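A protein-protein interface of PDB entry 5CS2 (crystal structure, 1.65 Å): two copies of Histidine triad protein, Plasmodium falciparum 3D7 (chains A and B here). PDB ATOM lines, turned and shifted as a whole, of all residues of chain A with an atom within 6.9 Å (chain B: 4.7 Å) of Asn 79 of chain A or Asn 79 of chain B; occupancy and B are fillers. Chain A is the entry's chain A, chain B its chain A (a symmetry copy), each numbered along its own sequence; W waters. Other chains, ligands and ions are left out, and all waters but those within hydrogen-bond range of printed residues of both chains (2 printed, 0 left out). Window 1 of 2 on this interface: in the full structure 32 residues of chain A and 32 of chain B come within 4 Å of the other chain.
Tyr 67 of chain A touches Asn 79 of chain B, and with the chains exchanged Asn 79 of chain A touches Tyr 67 of chain B. Tyr 67 of chain A touches Asn 83 of chain B, and with the chains exchanged Asn 83 of chain A touches Tyr 67 of chain B. Ile 75 of chain A touches Asn 79 of chain B, and with the chains exchanged Asn 79 of chain A touches Ile 75 of chain B. Ile 75 of chain A touches Leu 80 of chain B, and with the chains exchanged Leu 80 of chain A touches Ile 75 of chain B. Of the 12 pairs that touch across the chains among the printed residues, 11 have their exchanged pair printed and touching as well.
Printed residues of chain A that touch a printed residue of chain B: Tyr 67, Ile 75, Asn 79, Leu 80, Asn 83 and Ile 100. Of the 11 printed residues of chain B, 5 touch a printed residue of chain A. Printed residues of chain B that touch a printed residue of chain A: Tyr 67, Ile 75, Asn 79, Leu 80 and Asn 83. Hydrophobic or aromatic side chains of chain B within 4 Å of the printed part of chain A: Tyr 67, Ile 75 and Leu 80. Among the printed residues, no Asp or Glu carboxylate lies within 4 Å of a Lys or Arg side-chain nitrogen of the other chain.
Ile 8 of chain A touches none of the printed residues of chain B. Of the printed residues of chain B, Tyr 67 of chain A touches Asn 79 (3.8 Å) and Asn 83 (3.0 Å). Of chain B, only Tyr 67 (3.8 Å), Ile 75 (3.9 Å) and Asn 79 (3.3 Å) come within 4 Å of Asn 79 of chain A. Printed residues of chain B within 4 Å of Leu 80 of chain A: Ile 75. Printed residues of chain B within 4 Å of Asn 83 of chain A: Tyr 67 and Ile 75. Of the printed residues of chain A, Tyr 67 of chain B touches Asn 79 (3.8 Å), Asn 83 (3.0 Å) and Ile 100 (3.7 Å). Ile 78 of chain B touches none of the printed residues of chain A. Asn 79 of chain B touches just these residues of chain A: Tyr 67 (3.8 Å), Ile 75 (3.9 Å) and Asn 79 (3.3 Å). The nearest residue of chain A that does not touch Asn 79 of chain B is Leu 80 of chain A (6.0 Å). The nearest printed residue of chain A that does not touch Tyr 67 of chain B is Cys 82 of chain A (4.1 Å).
The side-chain amide oxygen (OD1) of Asn 79 of chain A lies close to the side-chain amide oxygen (OD1) of Asn 79 of chain B, 3.3 Å away. The side-chain amide nitrogen (ND2) of Asn 83 of chain A is in hydrogen-bond range of the backbone carbonyl oxygen (O) of Tyr 67 of chain B (3.0 Å). O of Tyr 67 of chain A lies within hydrogen-bond range of ND2 of Asn 83 of chain B, at 3.0 Å.
Water W1 lies within hydrogen-bond range of OD1 of Asn 79 of chain A, OH of Tyr 67 of chain B and SG of Cys 82 of chain A. Water W2 lies within hydrogen-bond range of the side-chain amide oxygen of Asn 79 of chain B (2.6 Å), the side-chain hydroxyl of Tyr 67 of chain A (2.8 Å) and the side-chain sulfur of Cys 82 of chain B (3.3 Å).
Among the printed residues, pairs that only touch across the chains: Ile 75 of chain A with Asn 83 of chain B, Asn 83 of chain A with Ile 75 of chain B, Ile 100 of chain A with Tyr 67 of chain B, Tyr 67 of chain A with Asn 79 of chain B, Asn 79 of chain A with Tyr 67 of chain B, Leu 80 of chain A with Ile 75 of chain B, Ile 75 of chain A with Leu 80 of chain B, Asn 79 of chain A with Ile 75 of chain B and Ile 75 of chain A with Asn 79 of chain B.
The side-chain hydroxyl (OH) of Tyr 67 of chain A is in hydrogen-bond range of the side-chain amide nitrogen (ND2) of Asn 79 of chain A (3.0 Å). O of Ile 75 of chain A sits at hydrogen-bond distance from ND2 of Asn 79 of chain A, 2.9 Å away. The side-chain amide nitrogen (ND2) of Asn 79 of chain B is in hydrogen-bond range of the backbone carbonyl oxygen (O) of Ile 75 of chain B (2.9 Å). The side-chain amide nitrogen of Asn 79 of chain B is in hydrogen-bond range of the side-chain hydroxyl of Tyr 67 of chain B.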
ATOM      1  N   ILE A   8      13.955  16.488   5.819  1.00  0.00           N
ATOM      2  CA  ILE A   8      14.898  17.182   4.937  1.00  0.00           C
ATOM      3  C   ILE A   8      14.892  18.686   5.304  1.00  0.00           C
ATOM      4  O   ILE A   8      15.954  19.280   5.466  1.00  0.00           O
ATOM      5  CB  ILE A   8      14.515  16.945   3.460  1.00  0.00           C
ATOM      6  CG1 ILE A   8      14.961  15.533   3.005  1.00  0.00           C
ATOM      7  CG2 ILE A   8      15.063  18.070   2.504  1.00  0.00           C
ATOM      8  CD1 ILE A   8      14.605  15.184   1.514  1.00  0.00           C
ATOM      9  N   LEU A  12      17.807  21.224   6.308  1.00  0.00           N
ATOM     10  CA  LEU A  12      18.054  22.446   5.536  1.00  0.00           C
ATOM     11  C   LEU A  12      17.907  23.688   6.419  1.00  0.00           C
ATOM     12  O   LEU A  12      18.119  24.814   5.941  1.00  0.00           O
ATOM     13  CB  LEU A  12      17.084  22.543   4.325  1.00  0.00           C
ATOM     14  CG  LEU A  12      17.204  21.500   3.200  1.00  0.00           C
ATOM     15  CD1 LEU A  12      16.045  21.577   2.270  1.00  0.00           C
ATOM     16  CD2 LEU A  12      18.477  21.691   2.417  1.00  0.00           C
ATOM     17  N   SER A  42      21.502  27.376   0.487  1.00  0.00           N
ATOM     18  CA  SER A  42      21.024  27.484  -0.895  1.00  0.00           C
ATOM     19  C   SER A  42      19.729  28.264  -0.992  1.00  0.00           C
ATOM     20  O   SER A  42      19.156  28.639   0.031  1.00  0.00           O
ATOM     21  CB  SER A  42      20.734  26.075  -1.426  1.00  0.00           C
ATOM     22  OG  SER A  42      21.794  25.176  -1.193  1.00  0.00           O
ATOM     23  N   LEU A  58      18.152  26.103  -8.596  1.00  0.00           N
ATOM     24  CA  LEU A  58      18.614  26.064  -7.206  1.00  0.00           C
ATOM     25  C   LEU A  58      20.065  26.504  -7.222  1.00  0.00           C
ATOM     26  O   LEU A  58      20.810  26.059  -8.096  1.00  0.00           O
ATOM     27  CB  LEU A  58      18.557  24.659  -6.596  1.00  0.00           C
ATOM     28  CG  LEU A  58      17.223  23.907  -6.704  1.00  0.00           C
ATOM     29  CD1 LEU A  58      17.279  22.654  -5.874  1.00  0.00           C
ATOM     30  CD2 LEU A  58      16.056  24.717  -6.193  1.00  0.00           C
ATOM     31  N   TYR A  67      31.023  23.021  -9.312  1.00  0.00           N
ATOM     32  CA  TYR A  67      30.442  22.082  -8.364  1.00  0.00           C
ATOM     33  C   TYR A  67      31.479  21.590  -7.352  1.00  0.00           C
ATOM     34  O   TYR A  67      31.176  21.419  -6.178  1.00  0.00           O
ATOM     35  CB  TYR A  67      29.835  20.899  -9.154  1.00  0.00           C
ATOM     36  CG  TYR A  67      28.963  19.971  -8.337  1.00  0.00           C
ATOM     37  CD1 TYR A  67      28.066  20.471  -7.395  1.00  0.00           C
ATOM     38  CD2 TYR A  67      28.985  18.595  -8.555  1.00  0.00           C
ATOM     39  CE1 TYR A  67      27.240  19.618  -6.657  1.00  0.00           C
ATOM     40  CE2 TYR A  67      28.171  17.732  -7.821  1.00  0.00           C
ATOM     41  CZ  TYR A  67      27.266  18.253  -6.908  1.00  0.00           C
ATOM     42  OH  TYR A  67      26.466  17.400  -6.186  1.00  0.00           O
ATOM     43  N   LEU A  70      32.186  23.477  -3.985  1.00  0.00           N
ATOM     44  CA  LEU A  70      31.286  23.376  -2.839  1.00  0.00           C
ATOM     45  C   LEU A  70      31.857  22.581  -1.697  1.00  0.00           C
ATOM     46  O   LEU A  70      32.521  21.568  -1.934  1.00  0.00           O
ATOM     47  CB  LEU A  70      29.901  22.796  -3.224  1.00  0.00           C
ATOM     48  CG  LEU A  70      29.074  23.420  -4.365  1.00  0.00           C
ATOM     49  CD1 LEU A  70      27.605  23.084  -4.164  1.00  0.00           C
ATOM     50  CD2 LEU A  70      29.204  24.913  -4.447  1.00  0.00           C
ATOM     51  N   GLU A  74      27.431  22.181   1.850  1.00  0.00           N
ATOM     52  CA  GLU A  74      26.743  22.797   0.712  1.00  0.00           C
ATOM     53  C   GLU A  74      26.236  21.758  -0.292  1.00  0.00           C
ATOM     54  O   GLU A  74      25.159  21.942  -0.855  1.00  0.00           O
ATOM     55  CB  GLU A  74      27.638  23.814  -0.022  1.00  0.00           C
ATOM     56  CG  GLU A  74      28.047  25.014   0.819  1.00  0.00           C
ATOM     57  CD  GLU A  74      28.992  25.969   0.109  1.00  0.00           C
ATOM     58  OE1 GLU A  74      30.042  25.506  -0.399  1.00  0.00           O
ATOM     59  OE2 GLU A  74      28.654  27.174   0.011  1.00  0.00           O
ATOM     60  N   ILE A  75      27.035  20.701  -0.553  1.00  0.00           N
ATOM     61  CA  ILE A  75      26.660  19.605  -1.472  1.00  0.00           C
ATOM     62  C   ILE A  75      25.418  18.932  -0.922  1.00  0.00           C
ATOM     63  O   ILE A  75      24.452  18.722  -1.652  1.00  0.00           O
ATOM     64  CB  ILE A  75      27.813  18.569  -1.692  1.00  0.00           C
ATOM     65  CG1 ILE A  75      29.014  19.244  -2.361  1.00  0.00           C
ATOM     66  CG2 ILE A  75      27.306  17.353  -2.552  1.00  0.00           C
ATOM     67  CD1 ILE A  75      30.353  18.522  -2.077  1.00  0.00           C
ATOM     68  N   ILE A  76      25.441  18.598   0.379  1.00  0.00           N
ATOM     69  CA  ILE A  76      24.278  17.965   1.001  1.00  0.00           C
ATOM     70  C   ILE A  76      23.058  18.877   0.939  1.00  0.00           C
ATOM     71  O   ILE A  76      21.959  18.430   0.586  1.00  0.00           O
ATOM     72  CB  ILE A  76      24.648  17.567   2.443  1.00  0.00           C
ATOM     73  CG1 ILE A  76      25.727  16.439   2.444  1.00  0.00           C
ATOM     74  CG2 ILE A  76      23.391  17.215   3.301  1.00  0.00           C
ATOM     75  CD1 ILE A  76      26.363  16.177   3.833  1.00  0.00           C
ATOM     76  N   ASP A  77      23.244  20.153   1.307  1.00  0.00           N
ATOM     77  CA  ASP A  77      22.138  21.109   1.343  1.00  0.00           C
ATOM     78  C   ASP A  77      21.466  21.263  -0.018  1.00  0.00           C
ATOM     79  O   ASP A  77      20.252  21.078  -0.125  1.00  0.00           O
ATOM     80  CB  ASP A  77      22.623  22.463   1.903  1.00  0.00           C
ATOM     81  CG  ASP A  77      21.500  23.474   2.117  1.00  0.00           C
ATOM     82  OD1 ASP A  77      20.894  23.902   1.116  1.00  0.00           O
ATOM     83  OD2 ASP A  77      21.267  23.877   3.295  1.00  0.00           O
ATOM     84  N   ILE A  78      22.237  21.572  -1.069  1.00  0.00           N
ATOM     85  CA  ILE A  78      21.660  21.834  -2.375  1.00  0.00           C
ATOM     86  C   ILE A  78      20.977  20.578  -2.972  1.00  0.00           C
ATOM     87  O   ILE A  78      19.971  20.707  -3.686  1.00  0.00           O
ATOM     88  CB  ILE A  78      22.638  22.520  -3.364  1.00  0.00           C
ATOM     89  CG1 ILE A  78      21.834  23.226  -4.478  1.00  0.00           C
ATOM     90  CG2 ILE A  78      23.634  21.513  -3.961  1.00  0.00           C
ATOM     91  CD1 ILE A  78      22.564  24.186  -5.393  1.00  0.00           C
ATOM     92  N   ASN A  79      21.500  19.395  -2.616  1.00  0.00           N
ATOM     93  CA  ASN A  79      20.973  18.146  -3.151  1.00  0.00           C
ATOM     94  C   ASN A  79      19.745  17.664  -2.416  1.00  0.00           C
ATOM     95  O   ASN A  79      18.830  17.153  -3.073  1.00  0.00           O
ATOM     96  CB  ASN A  79      22.049  17.106  -3.258  1.00  0.00           C
ATOM     97  CG  ASN A  79      22.858  17.382  -4.513  1.00  0.00           C
ATOM     98  OD1 ASN A  79      22.344  17.403  -5.640  1.00  0.00           O
ATOM     99  ND2 ASN A  79      24.106  17.764  -4.325  1.00  0.00           N
ATOM    100  N   LEU A  80      19.687  17.864  -1.106  1.00  0.00           N
ATOM    101  CA  LEU A  80      18.452  17.574  -0.356  1.00  0.00           C
ATOM    102  C   LEU A  80      17.350  18.544  -0.802  1.00  0.00           C
ATOM    103  O   LEU A  80      16.211  18.124  -0.998  1.00  0.00           O
ATOM    104  CB  LEU A  80      18.675  17.641   1.150  1.00  0.00           C
ATOM    105  CG  LEU A  80      19.594  16.568   1.760  1.00  0.00           C
ATOM    106  CD1 LEU A  80      19.732  16.797   3.251  1.00  0.00           C
ATOM    107  CD2 LEU A  80      19.086  15.135   1.484  1.00  0.00           C
ATOM    108  N   LEU A  81      17.704  19.836  -1.048  1.00  0.00           N
ATOM    109  CA  LEU A  81      16.731  20.807  -1.572  1.00  0.00           C
ATOM    110  C   LEU A  81      16.211  20.385  -2.953  1.00  0.00           C
ATOM    111  O   LEU A  81      15.029  20.495  -3.239  1.00  0.00           O
ATOM    112  CB  LEU A  81      17.377  22.224  -1.635  1.00  0.00           C
ATOM    113  CG  LEU A  81      16.453  23.324  -2.143  1.00  0.00           C
ATOM    114  CD1 LEU A  81      15.200  23.459  -1.231  1.00  0.00           C
ATOM    115  CD2 LEU A  81      17.176  24.657  -2.179  1.00  0.00           C
ATOM    116  N   CYS A  82      17.100  19.887  -3.821  1.00  0.00           N
ATOM    117  CA  CYS A  82      16.716  19.390  -5.127  1.00  0.00           C
ATOM    118  C   CYS A  82      15.672  18.283  -5.017  1.00  0.00           C
ATOM    119  O   CYS A  82      14.651  18.340  -5.712  1.00  0.00           O
ATOM    120  CB  CYS A  82      17.928  18.910  -5.918  1.00  0.00           C
ATOM    121  SG  CYS A  82      17.502  18.330  -7.572  1.00  0.00           S
ATOM    122  N   ASN A  83      15.955  17.276  -4.196  1.00  0.00           N
ATOM    123  CA  ASN A  83      15.031  16.138  -4.013  1.00  0.00           C
ATOM    124  C   ASN A  83      13.672  16.652  -3.478  1.00  0.00           C
ATOM    125  O   ASN A  83      12.630  16.299  -4.039  1.00  0.00           O
ATOM    126  CB  ASN A  83      15.653  15.113  -3.070  1.00  0.00           C
ATOM    127  CG  ASN A  83      14.923  13.806  -3.113  1.00  0.00           C
ATOM    128  OD1 ASN A  83      13.997  13.572  -2.337  1.00  0.00           O
ATOM    129  ND2 ASN A  83      15.364  12.914  -3.967  1.00  0.00           N
ATOM    130  N   PHE A  84      13.711  17.534  -2.462  1.00  0.00           N
ATOM    131  CA  PHE A  84      12.522  18.160  -1.868  1.00  0.00           C
ATOM    132  C   PHE A  84      11.739  18.913  -2.946  1.00  0.00           C
ATOM    133  O   PHE A  84      10.512  18.791  -3.010  1.00  0.00           O
ATOM    134  CB  PHE A  84      12.921  19.104  -0.729  1.00  0.00           C
ATOM    135  CG  PHE A  84      11.755  19.872  -0.130  1.00  0.00           C
ATOM    136  CD1 PHE A  84      10.849  19.240   0.725  1.00  0.00           C
ATOM    137  CD2 PHE A  84      11.518  21.198  -0.487  1.00  0.00           C
ATOM    138  CE1 PHE A  84       9.769  19.943   1.271  1.00  0.00           C
ATOM    139  CE2 PHE A  84      10.403  21.889   0.023  1.00  0.00           C
ATOM    140  CZ  PHE A  84       9.556  21.263   0.920  1.00  0.00           C
ATOM    141  N   ILE A 100      16.856  16.793 -14.420  1.00  0.00           N
ATOM    142  CA  ILE A 100      17.614  17.447 -13.366  1.00  0.00           C
ATOM    143  C   ILE A 100      19.027  17.599 -13.891  1.00  0.00           C
ATOM    144  O   ILE A 100      19.595  16.611 -14.363  1.00  0.00           O
ATOM    145  CB  ILE A 100      17.567  16.664 -12.043  1.00  0.00           C
ATOM    146  CG1 ILE A 100      16.089  16.328 -11.608  1.00  0.00           C
ATOM    147  CG2 ILE A 100      18.359  17.395 -10.949  1.00  0.00           C
ATOM    148  CD1 ILE A 100      16.075  15.208 -10.595  1.00  0.00           C
ATOM    149  N   ILE A 102      23.101  19.890 -13.926  1.00  0.00           N
ATOM    150  CA  ILE A 102      24.085  20.933 -13.607  1.00  0.00           C
ATOM    151  C   ILE A 102      24.964  21.110 -14.857  1.00  0.00           C
ATOM    152  O   ILE A 102      25.484  20.116 -15.370  1.00  0.00           O
ATOM    153  CB  ILE A 102      24.957  20.607 -12.370  1.00  0.00           C
ATOM    154  CG1 ILE A 102      24.101  20.317 -11.108  1.00  0.00           C
ATOM    155  CG2 ILE A 102      25.983  21.740 -12.100  1.00  0.00           C
ATOM    156  CD1 ILE A 102      24.959  19.946  -9.856  1.00  0.00           C
ATOM    157  N   ILE A 117      21.467  24.157 -10.091  1.00  0.00           N
ATOM    158  CA  ILE A 117      20.802  22.957 -10.583  1.00  0.00           C
ATOM    159  C   ILE A 117      19.522  23.383 -11.277  1.00  0.00           C
ATOM    160  O   ILE A 117      18.765  24.195 -10.721  1.00  0.00           O
ATOM    161  CB  ILE A 117      20.428  22.019  -9.399  1.00  0.00           C
ATOM    162  CG1 ILE A 117      21.660  21.552  -8.579  1.00  0.00           C
ATOM    163  CG2 ILE A 117      19.582  20.815  -9.909  1.00  0.00           C
ATOM    164  CD1 ILE A 117      21.379  20.704  -7.272  1.00  0.00           C
ATOM    165  N   TYR B  67      13.914   9.432  -8.431  1.00  0.00           N
ATOM    166  CA  TYR B  67      14.772  10.144  -7.496  1.00  0.00           C
ATOM    167  C   TYR B  67      14.082  10.352  -6.145  1.00  0.00           C
ATOM    168  O   TYR B  67      14.712  10.256  -5.100  1.00  0.00           O
ATOM    169  CB  TYR B  67      15.169  11.498  -8.128  1.00  0.00           C
ATOM    170  CG  TYR B  67      16.268  12.240  -7.400  1.00  0.00           C
ATOM    171  CD1 TYR B  67      17.378  11.566  -6.895  1.00  0.00           C
ATOM    172  CD2 TYR B  67      16.233  13.628  -7.277  1.00  0.00           C
ATOM    173  CE1 TYR B  67      18.409  12.253  -6.245  1.00  0.00           C
ATOM    174  CE2 TYR B  67      17.251  14.324  -6.625  1.00  0.00           C
ATOM    175  CZ  TYR B  67      18.359  13.637  -6.154  1.00  0.00           C
ATOM    176  OH  TYR B  67      19.360  14.325  -5.511  1.00  0.00           O
ATOM    177  N   ILE B  75      20.301   9.788  -0.876  1.00  0.00           N
ATOM    178  CA  ILE B  75      20.437  11.080  -1.582  1.00  0.00           C
ATOM    179  C   ILE B  75      21.807  11.650  -1.268  1.00  0.00           C
ATOM    180  O   ILE B  75      22.532  12.056  -2.172  1.00  0.00           O
ATOM    181  CB  ILE B  75      19.305  12.099  -1.220  1.00  0.00           C
ATOM    182  CG1 ILE B  75      17.941  11.557  -1.657  1.00  0.00           C
ATOM    183  CG2 ILE B  75      19.588  13.498  -1.880  1.00  0.00           C
ATOM    184  CD1 ILE B  75      16.764  12.147  -0.845  1.00  0.00           C
ATOM    185  N   ILE B  76      22.165  11.671   0.027  1.00  0.00           N
ATOM    186  CA  ILE B  76      23.478  12.182   0.423  1.00  0.00           C
ATOM    187  C   ILE B  76      24.598  11.351  -0.192  1.00  0.00           C
ATOM    188  O   ILE B  76      25.566  11.905  -0.729  1.00  0.00           O
ATOM    189  CB  ILE B  76      23.546  12.221   1.962  1.00  0.00           C
ATOM    190  CG1 ILE B  76      22.551  13.281   2.531  1.00  0.00           C
ATOM    191  CG2 ILE B  76      25.006  12.407   2.484  1.00  0.00           C
ATOM    192  CD1 ILE B  76      22.345  13.191   4.065  1.00  0.00           C
ATOM    193  N   ASP B  77      24.480  10.019  -0.095  1.00  0.00           N
ATOM    194  CA  ASP B  77      25.517   9.119  -0.596  1.00  0.00           C
ATOM    195  C   ASP B  77      25.770   9.309  -2.090  1.00  0.00           C
ATOM    196  O   ASP B  77      26.910   9.554  -2.491  1.00  0.00           O
ATOM    197  CB  ASP B  77      25.166   7.657  -0.252  1.00  0.00           C
ATOM    198  CG  ASP B  77      26.269   6.662  -0.607  1.00  0.00           C
ATOM    199  OD1 ASP B  77      26.549   6.499  -1.809  1.00  0.00           O
ATOM    200  OD2 ASP B  77      26.812   6.005   0.329  1.00  0.00           O
ATOM    201  N   ILE B  78      24.722   9.226  -2.920  1.00  0.00           N
ATOM    202  CA  ILE B  78      24.896   9.294  -4.359  1.00  0.00           C
ATOM    203  C   ILE B  78      25.424  10.677  -4.817  1.00  0.00           C
ATOM    204  O   ILE B  78      26.180  10.752  -5.796  1.00  0.00           O
ATOM    205  CB  ILE B  78      23.654   8.824  -5.161  1.00  0.00           C
ATOM    206  CG1 ILE B  78      24.084   8.423  -6.590  1.00  0.00           C
ATOM    207  CG2 ILE B  78      22.564   9.907  -5.201  1.00  0.00           C
ATOM    208  CD1 ILE B  78      23.092   7.678  -7.457  1.00  0.00           C
ATOM    209  N   ASN B  79      25.063  11.727  -4.062  1.00  0.00           N
ATOM    210  CA  ASN B  79      25.459  13.083  -4.420  1.00  0.00           C
ATOM    211  C   ASN B  79      26.861  13.423  -3.974  1.00  0.00           C
ATOM    212  O   ASN B  79      27.569  14.103  -4.726  1.00  0.00           O
ATOM    213  CB  ASN B  79      24.434  14.082  -3.973  1.00  0.00           C
ATOM    214  CG  ASN B  79      23.292  14.078  -4.975  1.00  0.00           C
ATOM    215  OD1 ASN B  79      23.464  14.336  -6.174  1.00  0.00           O
ATOM    216  ND2 ASN B  79      22.137  13.620  -4.534  1.00  0.00           N
ATOM    217  N   LEU B  80      27.282  12.926  -2.818  1.00  0.00           N
ATOM    218  CA  LEU B  80      28.688  13.076  -2.403  1.00  0.00           C
ATOM    219  C   LEU B  80      29.584  12.274  -3.355  1.00  0.00           C
ATOM    220  O   LEU B  80      30.636  12.767  -3.764  1.00  0.00           O
ATOM    221  CB  LEU B  80      28.900  12.653  -0.954  1.00  0.00           C
ATOM    222  CG  LEU B  80      28.230  13.523   0.123  1.00  0.00           C
ATOM    223  CD1 LEU B  80      28.513  12.950   1.497  1.00  0.00           C
ATOM    224  CD2 LEU B  80      28.686  14.997   0.055  1.00  0.00           C
ATOM    225  N   LEU B  81      29.131  11.064  -3.785  1.00  0.00           N
ATOM    226  CA  LEU B  81      29.882  10.275  -4.774  1.00  0.00           C
ATOM    227  C   LEU B  81      30.002  11.023  -6.108  1.00  0.00           C
ATOM    228  O   LEU B  81      31.050  11.023  -6.735  1.00  0.00           O
ATOM    229  CB  LEU B  81      29.197   8.889  -4.977  1.00  0.00           C
ATOM    230  CG  LEU B  81      29.900   7.970  -5.968  1.00  0.00           C
ATOM    231  CD1 LEU B  81      31.355   7.670  -5.507  1.00  0.00           C
ATOM    232  CD2 LEU B  81      29.152   6.658  -6.107  1.00  0.00           C
ATOM    233  N   CYS B  82      28.921  11.678  -6.548  1.00  0.00           N
ATOM    234  CA  CYS B  82      28.936  12.478  -7.757  1.00  0.00           C
ATOM    235  C   CYS B  82      30.005  13.565  -7.693  1.00  0.00           C
ATOM    236  O   CYS B  82      30.783  13.705  -8.642  1.00  0.00           O
ATOM    237  CB  CYS B  82      27.565  13.087  -8.036  1.00  0.00           C
ATOM    238  SG  CYS B  82      27.524  14.050  -9.561  1.00  0.00           S
ATOM    239  N   ASN B  83      30.001  14.343  -6.615  1.00  0.00           N
ATOM    240  CA  ASN B  83      30.978  15.438  -6.442  1.00  0.00           C
ATOM    241  C   ASN B  83      32.414  14.861  -6.450  1.00  0.00           C
ATOM    242  O   ASN B  83      33.265  15.369  -7.186  1.00  0.00           O
ATOM    243  CB  ASN B  83      30.684  16.194  -5.150  1.00  0.00           C
ATOM    244  CG  ASN B  83      31.416  17.500  -5.095  1.00  0.00           C
ATOM    245  OD1 ASN B  83      32.531  17.579  -4.581  1.00  0.00           O
ATOM    246  ND2 ASN B  83      30.782  18.549  -5.557  1.00  0.00           N
ATOM    247  N   ILE B 117      22.810   8.834 -12.133  1.00  0.00           N
ATOM    248  CA  ILE B 117      23.349  10.138 -12.500  1.00  0.00           C
ATOM    249  C   ILE B 117      24.364   9.929 -13.607  1.00  0.00           C
ATOM    250  O   ILE B 117      25.220   9.037 -13.494  1.00  0.00           O
ATOM    251  CB  ILE B 117      24.075  10.788 -11.287  1.00  0.00           C
ATOM    252  CG1 ILE B 117      23.143  11.009 -10.066  1.00  0.00           C
ATOM    253  CG2 ILE B 117      24.782  12.105 -11.722  1.00  0.00           C
ATOM    254  CD1 ILE B 117      23.813  11.540  -8.732  1.00  0.00           C
HETATM  255  O   HOH W   1      20.240  16.533  -6.964  1.00  0.00           O
HETATM  256  O   HOH W   2      25.135  15.561  -7.801  1.00  0.00           O
